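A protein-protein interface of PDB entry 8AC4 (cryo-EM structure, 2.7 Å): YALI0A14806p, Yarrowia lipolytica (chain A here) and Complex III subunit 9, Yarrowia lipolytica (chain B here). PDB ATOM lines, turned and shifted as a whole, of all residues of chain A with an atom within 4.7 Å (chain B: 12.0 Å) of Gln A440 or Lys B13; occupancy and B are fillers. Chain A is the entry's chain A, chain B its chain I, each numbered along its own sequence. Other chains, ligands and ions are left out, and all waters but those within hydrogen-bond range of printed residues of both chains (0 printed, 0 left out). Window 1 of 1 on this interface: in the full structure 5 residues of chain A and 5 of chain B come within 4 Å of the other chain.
No residue of chain B comes within 4 Å of Ala A437. No residue of chain B comes within 4 Å of Trp A438. No residue of chain B comes within 4 Å of Ala A439. Gln A440 touches one residue of chain B. No residue of chain B comes within 4 Å of Thr A442. Tyr A444 touches just one residue of chain B: Lys B13. Tyr B8 touches none of the printed residues of chain A. Of chain A, only Gln A440, Tyr A444 and Trp A474 come within 4 Å of Lys B13. Of the printed residues of chain A, Asn B15 touches Trp A474 (3.3 Å). Of the printed residues of chain A, Ser B16 touches Trp A474 (2.9 Å).
The side-chain amide oxygen (OD1) of Asn B9 sits at hydrogen-bond distance from the side-chain amino group (NZ) of Lys B13, 3.3 Å away. NH1 of Arg B14 lies within hydrogen-bond range of O of Asn B9 (3.3 Å). The backbone carbonyl oxygen (O) of Ser A374 sits at hydrogen-bond distance from the side-chain amide nitrogen (NE2) of Gln A440 (2.8 Å). The backbone carbonyl oxygen (O) of Ala A439 sits at hydrogen-bond distance from the backbone NH (N) of Tyr A444, at 3.0 Å. The backbone carbonyl oxygen (O) of Tyr B8 lies within hydrogen-bond range of the backbone NH (N) of Lys B13, 2.9 Å away.
The backbone carbonyl oxygen (O) of Trp A474 sits close to the backbone NH (N) of Asn B15. The side-chain amide oxygen of Gln A440 lies within hydrogen-bond range of the side-chain amino group of Lys B13 (3.1 Å). O of Trp A474 lies within hydrogen-bond range of N of Ser B16.
Among the printed residues, pairs that only touch across the chains: Tyr A444 with Lys B13, Trp A474 with Lys B13 and Trp A474 with Arg B14.
Of the 19 printed residues of chain B, 4 touch a printed residue of chain A. Along chain B the printed residues that touch a printed residue of chain A span positions 13 to 16. Hydrophobic or aromatic side chains of chain A within 4 Å of the printed part of chain B: Tyr A444 and Trp A474. Among the printed residues, 6 pairs touch across the chains. Among the printed residues, no Asp or Glu carboxylate lies within 4 Å of a Lys or Arg side-chain nitrogen of the other chain.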
ATOM      1  N   SER A 374     -28.658 -17.655   4.888  1.00  0.00           N
ATOM      2  CA  SER A 374     -27.937 -18.786   4.332  1.00  0.00           C
ATOM      3  C   SER A 374     -28.915 -19.899   4.008  1.00  0.00           C
ATOM      4  O   SER A 374     -28.704 -20.600   3.028  1.00  0.00           O
ATOM      5  CB  SER A 374     -26.869 -19.313   5.249  1.00  0.00           C
ATOM      6  OG  SER A 374     -25.831 -18.363   5.412  1.00  0.00           O
ATOM      7  N   ARG A 436     -27.970 -16.107  -0.976  1.00  0.00           N
ATOM      8  CA  ARG A 436     -27.656 -17.314  -0.214  1.00  0.00           C
ATOM      9  C   ARG A 436     -26.172 -17.659  -0.367  1.00  0.00           C
ATOM     10  O   ARG A 436     -25.523 -18.055   0.595  1.00  0.00           O
ATOM     11  CB  ARG A 436     -28.478 -18.536  -0.636  1.00  0.00           C
ATOM     12  CG  ARG A 436     -29.955 -18.516  -0.273  1.00  0.00           C
ATOM     13  CD  ARG A 436     -30.748 -19.431  -1.211  1.00  0.00           C
ATOM     14  NE  ARG A 436     -30.409 -20.780  -0.804  1.00  0.00           N
ATOM     15  CZ  ARG A 436     -30.863 -21.312   0.320  1.00  0.00           C
ATOM     16  NH1 ARG A 436     -31.688 -20.617   1.087  1.00  0.00           N
ATOM     17  NH2 ARG A 436     -30.497 -22.526   0.674  1.00  0.00           N
ATOM     18  N   ALA A 437     -25.623 -17.520  -1.575  1.00  0.00           N
ATOM     19  CA  ALA A 437     -24.238 -17.909  -1.758  1.00  0.00           C
ATOM     20  C   ALA A 437     -23.339 -17.016  -0.917  1.00  0.00           C
ATOM     21  O   ALA A 437     -22.350 -17.495  -0.366  1.00  0.00           O
ATOM     22  CB  ALA A 437     -23.853 -17.834  -3.205  1.00  0.00           C
ATOM     23  N   TRP A 438     -23.671 -15.722  -0.885  1.00  0.00           N
ATOM     24  CA  TRP A 438     -22.815 -14.750  -0.241  1.00  0.00           C
ATOM     25  C   TRP A 438     -22.874 -15.008   1.254  1.00  0.00           C
ATOM     26  O   TRP A 438     -21.838 -14.998   1.912  1.00  0.00           O
ATOM     27  CB  TRP A 438     -23.216 -13.316  -0.607  1.00  0.00           C
ATOM     28  CG  TRP A 438     -22.503 -12.288   0.211  1.00  0.00           C
ATOM     29  CD1 TRP A 438     -21.286 -11.728  -0.048  1.00  0.00           C
ATOM     30  CD2 TRP A 438     -22.978 -11.696   1.432  1.00  0.00           C
ATOM     31  NE1 TRP A 438     -20.956 -10.856   0.954  1.00  0.00           N
ATOM     32  CE2 TRP A 438     -21.979 -10.799   1.864  1.00  0.00           C
ATOM     33  CE3 TRP A 438     -24.139 -11.844   2.202  1.00  0.00           C
ATOM     34  CZ2 TRP A 438     -22.101 -10.073   3.047  1.00  0.00           C
ATOM     35  CZ3 TRP A 438     -24.260 -11.129   3.372  1.00  0.00           C
ATOM     36  CH2 TRP A 438     -23.254 -10.249   3.782  1.00  0.00           C
ATOM     37  N   ALA A 439     -24.087 -15.252   1.762  1.00  0.00           N
ATOM     38  CA  ALA A 439     -24.267 -15.406   3.196  1.00  0.00           C
ATOM     39  C   ALA A 439     -23.553 -16.659   3.682  1.00  0.00           C
ATOM     40  O   ALA A 439     -23.007 -16.696   4.780  1.00  0.00           O
ATOM     41  CB  ALA A 439     -25.728 -15.458   3.536  1.00  0.00           C
ATOM     42  N   GLN A 440     -23.563 -17.687   2.837  1.00  0.00           N
ATOM     43  CA  GLN A 440     -23.000 -18.963   3.223  1.00  0.00           C
ATOM     44  C   GLN A 440     -21.483 -18.877   3.272  1.00  0.00           C
ATOM     45  O   GLN A 440     -20.858 -19.671   3.970  1.00  0.00           O
ATOM     46  CB  GLN A 440     -23.448 -20.034   2.248  1.00  0.00           C
ATOM     47  CG  GLN A 440     -24.767 -20.638   2.669  1.00  0.00           C
ATOM     48  CD  GLN A 440     -25.277 -21.523   1.565  1.00  0.00           C
ATOM     49  OE1 GLN A 440     -24.518 -21.993   0.719  1.00  0.00           O
ATOM     50  NE2 GLN A 440     -26.582 -21.717   1.526  1.00  0.00           N
ATOM     51  N   LYS A 441     -20.901 -17.907   2.560  1.00  0.00           N
ATOM     52  CA  LYS A 441     -19.452 -17.792   2.578  1.00  0.00           C
ATOM     53  C   LYS A 441     -18.982 -16.720   3.559  1.00  0.00           C
ATOM     54  O   LYS A 441     -17.818 -16.728   3.957  1.00  0.00           O
ATOM     55  CB  LYS A 441     -18.856 -17.703   1.173  1.00  0.00           C
ATOM     56  CG  LYS A 441     -18.911 -16.336   0.519  1.00  0.00           C
ATOM     57  CD  LYS A 441     -18.064 -16.271  -0.715  1.00  0.00           C
ATOM     58  CE  LYS A 441     -17.510 -14.882  -0.902  1.00  0.00           C
ATOM     59  NZ  LYS A 441     -17.572 -14.470  -2.324  1.00  0.00           N
ATOM     60  N   THR A 442     -19.887 -15.831   3.977  1.00  0.00           N
ATOM     61  CA  THR A 442     -19.498 -14.629   4.691  1.00  0.00           C
ATOM     62  C   THR A 442     -20.063 -14.628   6.104  1.00  0.00           C
ATOM     63  O   THR A 442     -19.456 -14.065   7.006  1.00  0.00           O
ATOM     64  CB  THR A 442     -20.016 -13.399   3.944  1.00  0.00           C
ATOM     65  OG1 THR A 442     -19.459 -13.437   2.630  1.00  0.00           O
ATOM     66  CG2 THR A 442     -19.680 -12.090   4.622  1.00  0.00           C
ATOM     67  N   TYR A 444     -22.175 -17.552   7.484  1.00  0.00           N
ATOM     68  CA  TYR A 444     -22.562 -18.805   8.094  1.00  0.00           C
ATOM     69  C   TYR A 444     -21.364 -19.377   8.830  1.00  0.00           C
ATOM     70  O   TYR A 444     -20.314 -19.537   8.221  1.00  0.00           O
ATOM     71  CB  TYR A 444     -23.026 -19.815   7.047  1.00  0.00           C
ATOM     72  CG  TYR A 444     -23.769 -20.923   7.731  1.00  0.00           C
ATOM     73  CD1 TYR A 444     -25.039 -20.673   8.226  1.00  0.00           C
ATOM     74  CD2 TYR A 444     -23.195 -22.166   7.965  1.00  0.00           C
ATOM     75  CE1 TYR A 444     -25.756 -21.645   8.897  1.00  0.00           C
ATOM     76  CE2 TYR A 444     -23.897 -23.151   8.648  1.00  0.00           C
ATOM     77  CZ  TYR A 444     -25.176 -22.881   9.123  1.00  0.00           C
ATOM     78  OH  TYR A 444     -25.897 -23.824   9.799  1.00  0.00           O
ATOM     79  N   TRP A 474     -29.799 -27.383  10.211  1.00  0.00           N
ATOM     80  CA  TRP A 474     -29.503 -27.282   8.798  1.00  0.00           C
ATOM     81  C   TRP A 474     -28.172 -27.969   8.513  1.00  0.00           C
ATOM     82  O   TRP A 474     -28.228 -29.003   7.833  1.00  0.00           O
ATOM     83  CB  TRP A 474     -29.439 -25.819   8.396  1.00  0.00           C
ATOM     84  CG  TRP A 474     -29.288 -25.542   6.935  1.00  0.00           C
ATOM     85  CD1 TRP A 474     -30.272 -25.578   5.993  1.00  0.00           C
ATOM     86  CD2 TRP A 474     -28.110 -25.071   6.261  1.00  0.00           C
ATOM     87  NE1 TRP A 474     -29.787 -25.173   4.780  1.00  0.00           N
ATOM     88  CE2 TRP A 474     -28.461 -24.864   4.908  1.00  0.00           C
ATOM     89  CE3 TRP A 474     -26.804 -24.783   6.664  1.00  0.00           C
ATOM     90  CZ2 TRP A 474     -27.549 -24.399   3.958  1.00  0.00           C
ATOM     91  CZ3 TRP A 474     -25.897 -24.316   5.732  1.00  0.00           C
ATOM     92  CH2 TRP A 474     -26.266 -24.137   4.391  1.00  0.00           C
ATOM     93  N   ALA B   4      -9.964 -27.710  -0.114  1.00  0.00           N
ATOM     94  CA  ALA B   4     -10.259 -27.377   1.393  1.00  0.00           C
ATOM     95  C   ALA B   4     -11.580 -26.649   1.687  1.00  0.00           C
ATOM     96  O   ALA B   4     -12.327 -27.055   2.587  1.00  0.00           O
ATOM     97  CB  ALA B   4      -9.094 -26.640   2.008  1.00  0.00           C
ATOM     98  N   THR B   5     -11.825 -25.520   1.004  1.00  0.00           N
ATOM     99  CA  THR B   5     -13.127 -24.881   0.934  1.00  0.00           C
ATOM    100  C   THR B   5     -14.172 -25.858   0.403  1.00  0.00           C
ATOM    101  O   THR B   5     -15.284 -25.917   0.929  1.00  0.00           O
ATOM    102  CB  THR B   5     -13.043 -23.670   0.002  1.00  0.00           C
ATOM    103  OG1 THR B   5     -12.053 -22.814   0.572  1.00  0.00           O
ATOM    104  CG2 THR B   5     -14.357 -22.942  -0.170  1.00  0.00           C
ATOM    105  N   THR B   6     -13.809 -26.603  -0.650  1.00  0.00           N
ATOM    106  CA  THR B   6     -14.716 -27.567  -1.250  1.00  0.00           C
ATOM    107  C   THR B   6     -15.097 -28.602  -0.203  1.00  0.00           C
ATOM    108  O   THR B   6     -16.276 -28.859   0.018  1.00  0.00           O
ATOM    109  CB  THR B   6     -14.087 -28.248  -2.464  1.00  0.00           C
ATOM    110  OG1 THR B   6     -13.860 -27.203  -3.409  1.00  0.00           O
ATOM    111  CG2 THR B   6     -14.980 -29.317  -3.052  1.00  0.00           C
ATOM    112  N   PHE B   7     -14.085 -29.152   0.466  1.00  0.00           N
ATOM    113  CA  PHE B   7     -14.348 -30.153   1.477  1.00  0.00           C
ATOM    114  C   PHE B   7     -15.266 -29.584   2.555  1.00  0.00           C
ATOM    115  O   PHE B   7     -16.226 -30.241   2.959  1.00  0.00           O
ATOM    116  CB  PHE B   7     -13.049 -30.733   2.030  1.00  0.00           C
ATOM    117  CG  PHE B   7     -13.253 -32.053   2.724  1.00  0.00           C
ATOM    118  CD1 PHE B   7     -13.645 -32.104   4.057  1.00  0.00           C
ATOM    119  CD2 PHE B   7     -13.075 -33.245   2.037  1.00  0.00           C
ATOM    120  CE1 PHE B   7     -13.840 -33.321   4.697  1.00  0.00           C
ATOM    121  CE2 PHE B   7     -13.279 -34.462   2.674  1.00  0.00           C
ATOM    122  CZ  PHE B   7     -13.660 -34.498   4.001  1.00  0.00           C
ATOM    123  N   TYR B   8     -14.970 -28.364   3.006  1.00  0.00           N
ATOM    124  CA  TYR B   8     -15.786 -27.734   4.024  1.00  0.00           C
ATOM    125  C   TYR B   8     -17.234 -27.619   3.556  1.00  0.00           C
ATOM    126  O   TYR B   8     -18.148 -27.998   4.287  1.00  0.00           O
ATOM    127  CB  TYR B   8     -15.227 -26.368   4.429  1.00  0.00           C
ATOM    128  CG  TYR B   8     -16.160 -25.665   5.372  1.00  0.00           C
ATOM    129  CD1 TYR B   8     -16.142 -25.964   6.728  1.00  0.00           C
ATOM    130  CD2 TYR B   8     -17.115 -24.778   4.899  1.00  0.00           C
ATOM    131  CE1 TYR B   8     -17.038 -25.376   7.606  1.00  0.00           C
ATOM    132  CE2 TYR B   8     -18.016 -24.179   5.767  1.00  0.00           C
ATOM    133  CZ  TYR B   8     -17.971 -24.471   7.124  1.00  0.00           C
ATOM    134  OH  TYR B   8     -18.847 -23.883   7.990  1.00  0.00           O
ATOM    135  N   ASN B   9     -17.419 -27.076   2.345  1.00  0.00           N
ATOM    136  CA  ASN B   9     -18.740 -26.772   1.811  1.00  0.00           C
ATOM    137  C   ASN B   9     -19.601 -28.018   1.651  1.00  0.00           C
ATOM    138  O   ASN B   9     -20.800 -27.978   1.921  1.00  0.00           O
ATOM    139  CB  ASN B   9     -18.675 -26.060   0.469  1.00  0.00           C
ATOM    140  CG  ASN B   9     -18.370 -24.597   0.657  1.00  0.00           C
ATOM    141  OD1 ASN B   9     -18.747 -24.008   1.667  1.00  0.00           O
ATOM    142  ND2 ASN B   9     -17.666 -24.017  -0.299  1.00  0.00           N
ATOM    143  N   VAL B  10     -18.979 -29.125   1.248  1.00  0.00           N
ATOM    144  CA  VAL B  10     -19.695 -30.360   1.002  1.00  0.00           C
ATOM    145  C   VAL B  10     -19.993 -31.109   2.298  1.00  0.00           C
ATOM    146  O   VAL B  10     -21.134 -31.499   2.511  1.00  0.00           O
ATOM    147  CB  VAL B  10     -18.950 -31.222  -0.025  1.00  0.00           C
ATOM    148  CG1 VAL B  10     -19.648 -32.552  -0.235  1.00  0.00           C
ATOM    149  CG2 VAL B  10     -18.848 -30.466  -1.336  1.00  0.00           C
ATOM    150  N   PHE B  11     -19.005 -31.306   3.170  1.00  0.00           N
ATOM    151  CA  PHE B  11     -19.219 -32.268   4.239  1.00  0.00           C
ATOM    152  C   PHE B  11     -19.476 -31.605   5.582  1.00  0.00           C
ATOM    153  O   PHE B  11     -19.878 -32.278   6.530  1.00  0.00           O
ATOM    154  CB  PHE B  11     -18.028 -33.214   4.344  1.00  0.00           C
ATOM    155  CG  PHE B  11     -17.847 -34.041   3.104  1.00  0.00           C
ATOM    156  CD1 PHE B  11     -18.689 -35.112   2.834  1.00  0.00           C
ATOM    157  CD2 PHE B  11     -16.864 -33.721   2.178  1.00  0.00           C
ATOM    158  CE1 PHE B  11     -18.533 -35.864   1.679  1.00  0.00           C
ATOM    159  CE2 PHE B  11     -16.705 -34.475   1.024  1.00  0.00           C
ATOM    160  CZ  PHE B  11     -17.539 -35.547   0.778  1.00  0.00           C
ATOM    161  N   VAL B  12     -19.206 -30.306   5.691  1.00  0.00           N
ATOM    162  CA  VAL B  12     -19.142 -29.755   7.031  1.00  0.00           C
ATOM    163  C   VAL B  12     -20.163 -28.646   7.226  1.00  0.00           C
ATOM    164  O   VAL B  12     -20.795 -28.585   8.271  1.00  0.00           O
ATOM    165  CB  VAL B  12     -17.716 -29.313   7.386  1.00  0.00           C
ATOM    166  CG1 VAL B  12     -17.655 -28.769   8.801  1.00  0.00           C
ATOM    167  CG2 VAL B  12     -16.771 -30.490   7.230  1.00  0.00           C
ATOM    168  N   LYS B  13     -20.309 -27.776   6.231  1.00  0.00           N
ATOM    169  CA  LYS B  13     -21.117 -26.574   6.364  1.00  0.00           C
ATOM    170  C   LYS B  13     -22.539 -26.901   6.831  1.00  0.00           C
ATOM    171  O   LYS B  13     -23.031 -26.282   7.766  1.00  0.00           O
ATOM    172  CB  LYS B  13     -21.099 -25.819   5.035  1.00  0.00           C
ATOM    173  CG  LYS B  13     -22.037 -24.631   4.915  1.00  0.00           C
ATOM    174  CD  LYS B  13     -21.757 -23.777   3.681  1.00  0.00           C
ATOM    175  CE  LYS B  13     -22.395 -24.287   2.401  1.00  0.00           C
ATOM    176  NZ  LYS B  13     -21.931 -23.548   1.198  1.00  0.00           N
ATOM    177  N   ARG B  14     -23.215 -27.839   6.169  1.00  0.00           N
ATOM    178  CA  ARG B  14     -24.548 -28.232   6.594  1.00  0.00           C
ATOM    179  C   ARG B  14     -24.421 -29.274   7.699  1.00  0.00           C
ATOM    180  O   ARG B  14     -23.706 -30.244   7.518  1.00  0.00           O
ATOM    181  CB  ARG B  14     -25.313 -28.827   5.411  1.00  0.00           C
ATOM    182  CG  ARG B  14     -25.788 -27.786   4.413  1.00  0.00           C
ATOM    183  CD  ARG B  14     -26.027 -28.441   3.071  1.00  0.00           C
ATOM    184  NE  ARG B  14     -26.219 -27.421   2.053  1.00  0.00           N
ATOM    185  CZ  ARG B  14     -25.246 -26.902   1.313  1.00  0.00           C
ATOM    186  NH1 ARG B  14     -23.998 -27.317   1.459  1.00  0.00           N
ATOM    187  NH2 ARG B  14     -25.527 -25.968   0.423  1.00  0.00           N
ATOM    188  N   ASN B  15     -25.098 -29.079   8.831  1.00  0.00           N
ATOM    189  CA  ASN B  15     -25.007 -30.040   9.914  1.00  0.00           C
ATOM    190  C   ASN B  15     -25.628 -31.372   9.502  1.00  0.00           C
ATOM    191  O   ASN B  15     -25.151 -32.426   9.899  1.00  0.00           O
ATOM    192  CB  ASN B  15     -25.701 -29.545  11.179  1.00  0.00           C
ATOM    193  CG  ASN B  15     -25.243 -30.309  12.398  1.00  0.00           C
ATOM    194  OD1 ASN B  15     -24.046 -30.529  12.563  1.00  0.00           O
ATOM    195  ND2 ASN B  15     -26.167 -30.687  13.268  1.00  0.00           N
ATOM    196  N   SER B  16     -26.672 -31.332   8.679  1.00  0.00           N
ATOM    197  CA  SER B  16     -27.220 -32.576   8.170  1.00  0.00           C
ATOM    198  C   SER B  16     -26.129 -33.378   7.457  1.00  0.00           C
ATOM    199  O   SER B  16     -26.047 -34.586   7.623  1.00  0.00           O
ATOM    200  CB  SER B  16     -28.385 -32.315   7.275  1.00  0.00           C
ATOM    201  OG  SER B  16     -27.990 -31.468   6.213  1.00  0.00           O
ATOM    202  N   ALA B  17     -25.288 -32.703   6.669  1.00  0.00           N
ATOM    203  CA  ALA B  17     -24.225 -33.388   5.952  1.00  0.00           C
ATOM    204  C   ALA B  17     -23.117 -33.832   6.904  1.00  0.00           C
ATOM    205  O   ALA B  17     -22.500 -34.874   6.702  1.00  0.00           O
ATOM    206  CB  ALA B  17     -23.683 -32.487   4.886  1.00  0.00           C
ATOM    207  N   PHE B  18     -22.829 -32.998   7.901  1.00  0.00           N
ATOM    208  CA  PHE B  18     -21.779 -33.298   8.855  1.00  0.00           C
ATOM    209  C   PHE B  18     -22.151 -34.523   9.675  1.00  0.00           C
ATOM    210  O   PHE B  18     -21.314 -35.391   9.884  1.00  0.00           O
ATOM    211  CB  PHE B  18     -21.590 -32.092   9.763  1.00  0.00           C
ATOM    212  CG  PHE B  18     -20.386 -32.123  10.660  1.00  0.00           C
ATOM    213  CD1 PHE B  18     -19.125 -32.403  10.149  1.00  0.00           C
ATOM    214  CD2 PHE B  18     -20.509 -31.794  12.005  1.00  0.00           C
ATOM    215  CE1 PHE B  18     -18.015 -32.402  10.982  1.00  0.00           C
ATOM    216  CE2 PHE B  18     -19.391 -31.770  12.831  1.00  0.00           C
ATOM    217  CZ  PHE B  18     -18.145 -32.082  12.319  1.00  0.00           C
ATOM    218  N   VAL B  19     -23.401 -34.571  10.136  1.00  0.00           N
ATOM    219  CA  VAL B  19     -23.836 -35.692  10.941  1.00  0.00           C
ATOM    220  C   VAL B  19     -23.870 -36.935  10.061  1.00  0.00           C
ATOM    221  O   VAL B  19     -23.468 -37.996  10.511  1.00  0.00           O
ATOM    222  CB  VAL B  19     -25.180 -35.413  11.635  1.00  0.00           C
ATOM    223  CG1 VAL B  19     -25.840 -36.695  12.123  1.00  0.00           C
ATOM    224  CG2 VAL B  19     -25.002 -34.429  12.784  1.00  0.00           C
ATOM    225  N   ALA B  20     -24.318 -36.794   8.806  1.00  0.00           N
ATOM    226  CA  ALA B  20     -24.331 -37.929   7.895  1.00  0.00           C
ATOM    227  C   ALA B  20     -22.919 -38.463   7.666  1.00  0.00           C
ATOM    228  O   ALA B  20     -22.733 -39.675   7.624  1.00  0.00           O
ATOM    229  CB  ALA B  20     -25.025 -37.602   6.596  1.00  0.00           C
ATOM    230  N   THR B  21     -21.938 -37.563   7.534  1.00  0.00           N
ATOM    231  CA  THR B  21     -20.554 -37.949   7.303  1.00  0.00           C
ATOM    232  C   THR B  21     -19.986 -38.651   8.532  1.00  0.00           C
ATOM    233  O   THR B  21     -19.248 -39.619   8.394  1.00  0.00           O
ATOM    234  CB  THR B  21     -19.716 -36.725   6.927  1.00  0.00           C
ATOM    235  OG1 THR B  21     -20.323 -36.186   5.755  1.00  0.00           O
ATOM    236  CG2 THR B  21     -18.263 -37.044   6.654  1.00  0.00           C
ATOM    237  N   ILE B  22     -20.312 -38.139   9.724  1.00  0.00           N
ATOM    238  CA  ILE B  22     -19.843 -38.713  10.975  1.00  0.00           C
ATOM    239  C   ILE B  22     -20.395 -40.131  11.107  1.00  0.00           C
ATOM    240  O   ILE B  22     -19.632 -41.033  11.421  1.00  0.00           O
ATOM    241  CB  ILE B  22     -20.195 -37.808  12.179  1.00  0.00           C
ATOM    242  CG1 ILE B  22     -19.290 -36.574  12.241  1.00  0.00           C
ATOM    243  CG2 ILE B  22     -20.194 -38.572  13.501  1.00  0.00           C
ATOM    244  CD1 ILE B  22     -19.892 -35.408  12.993  1.00  0.00           C
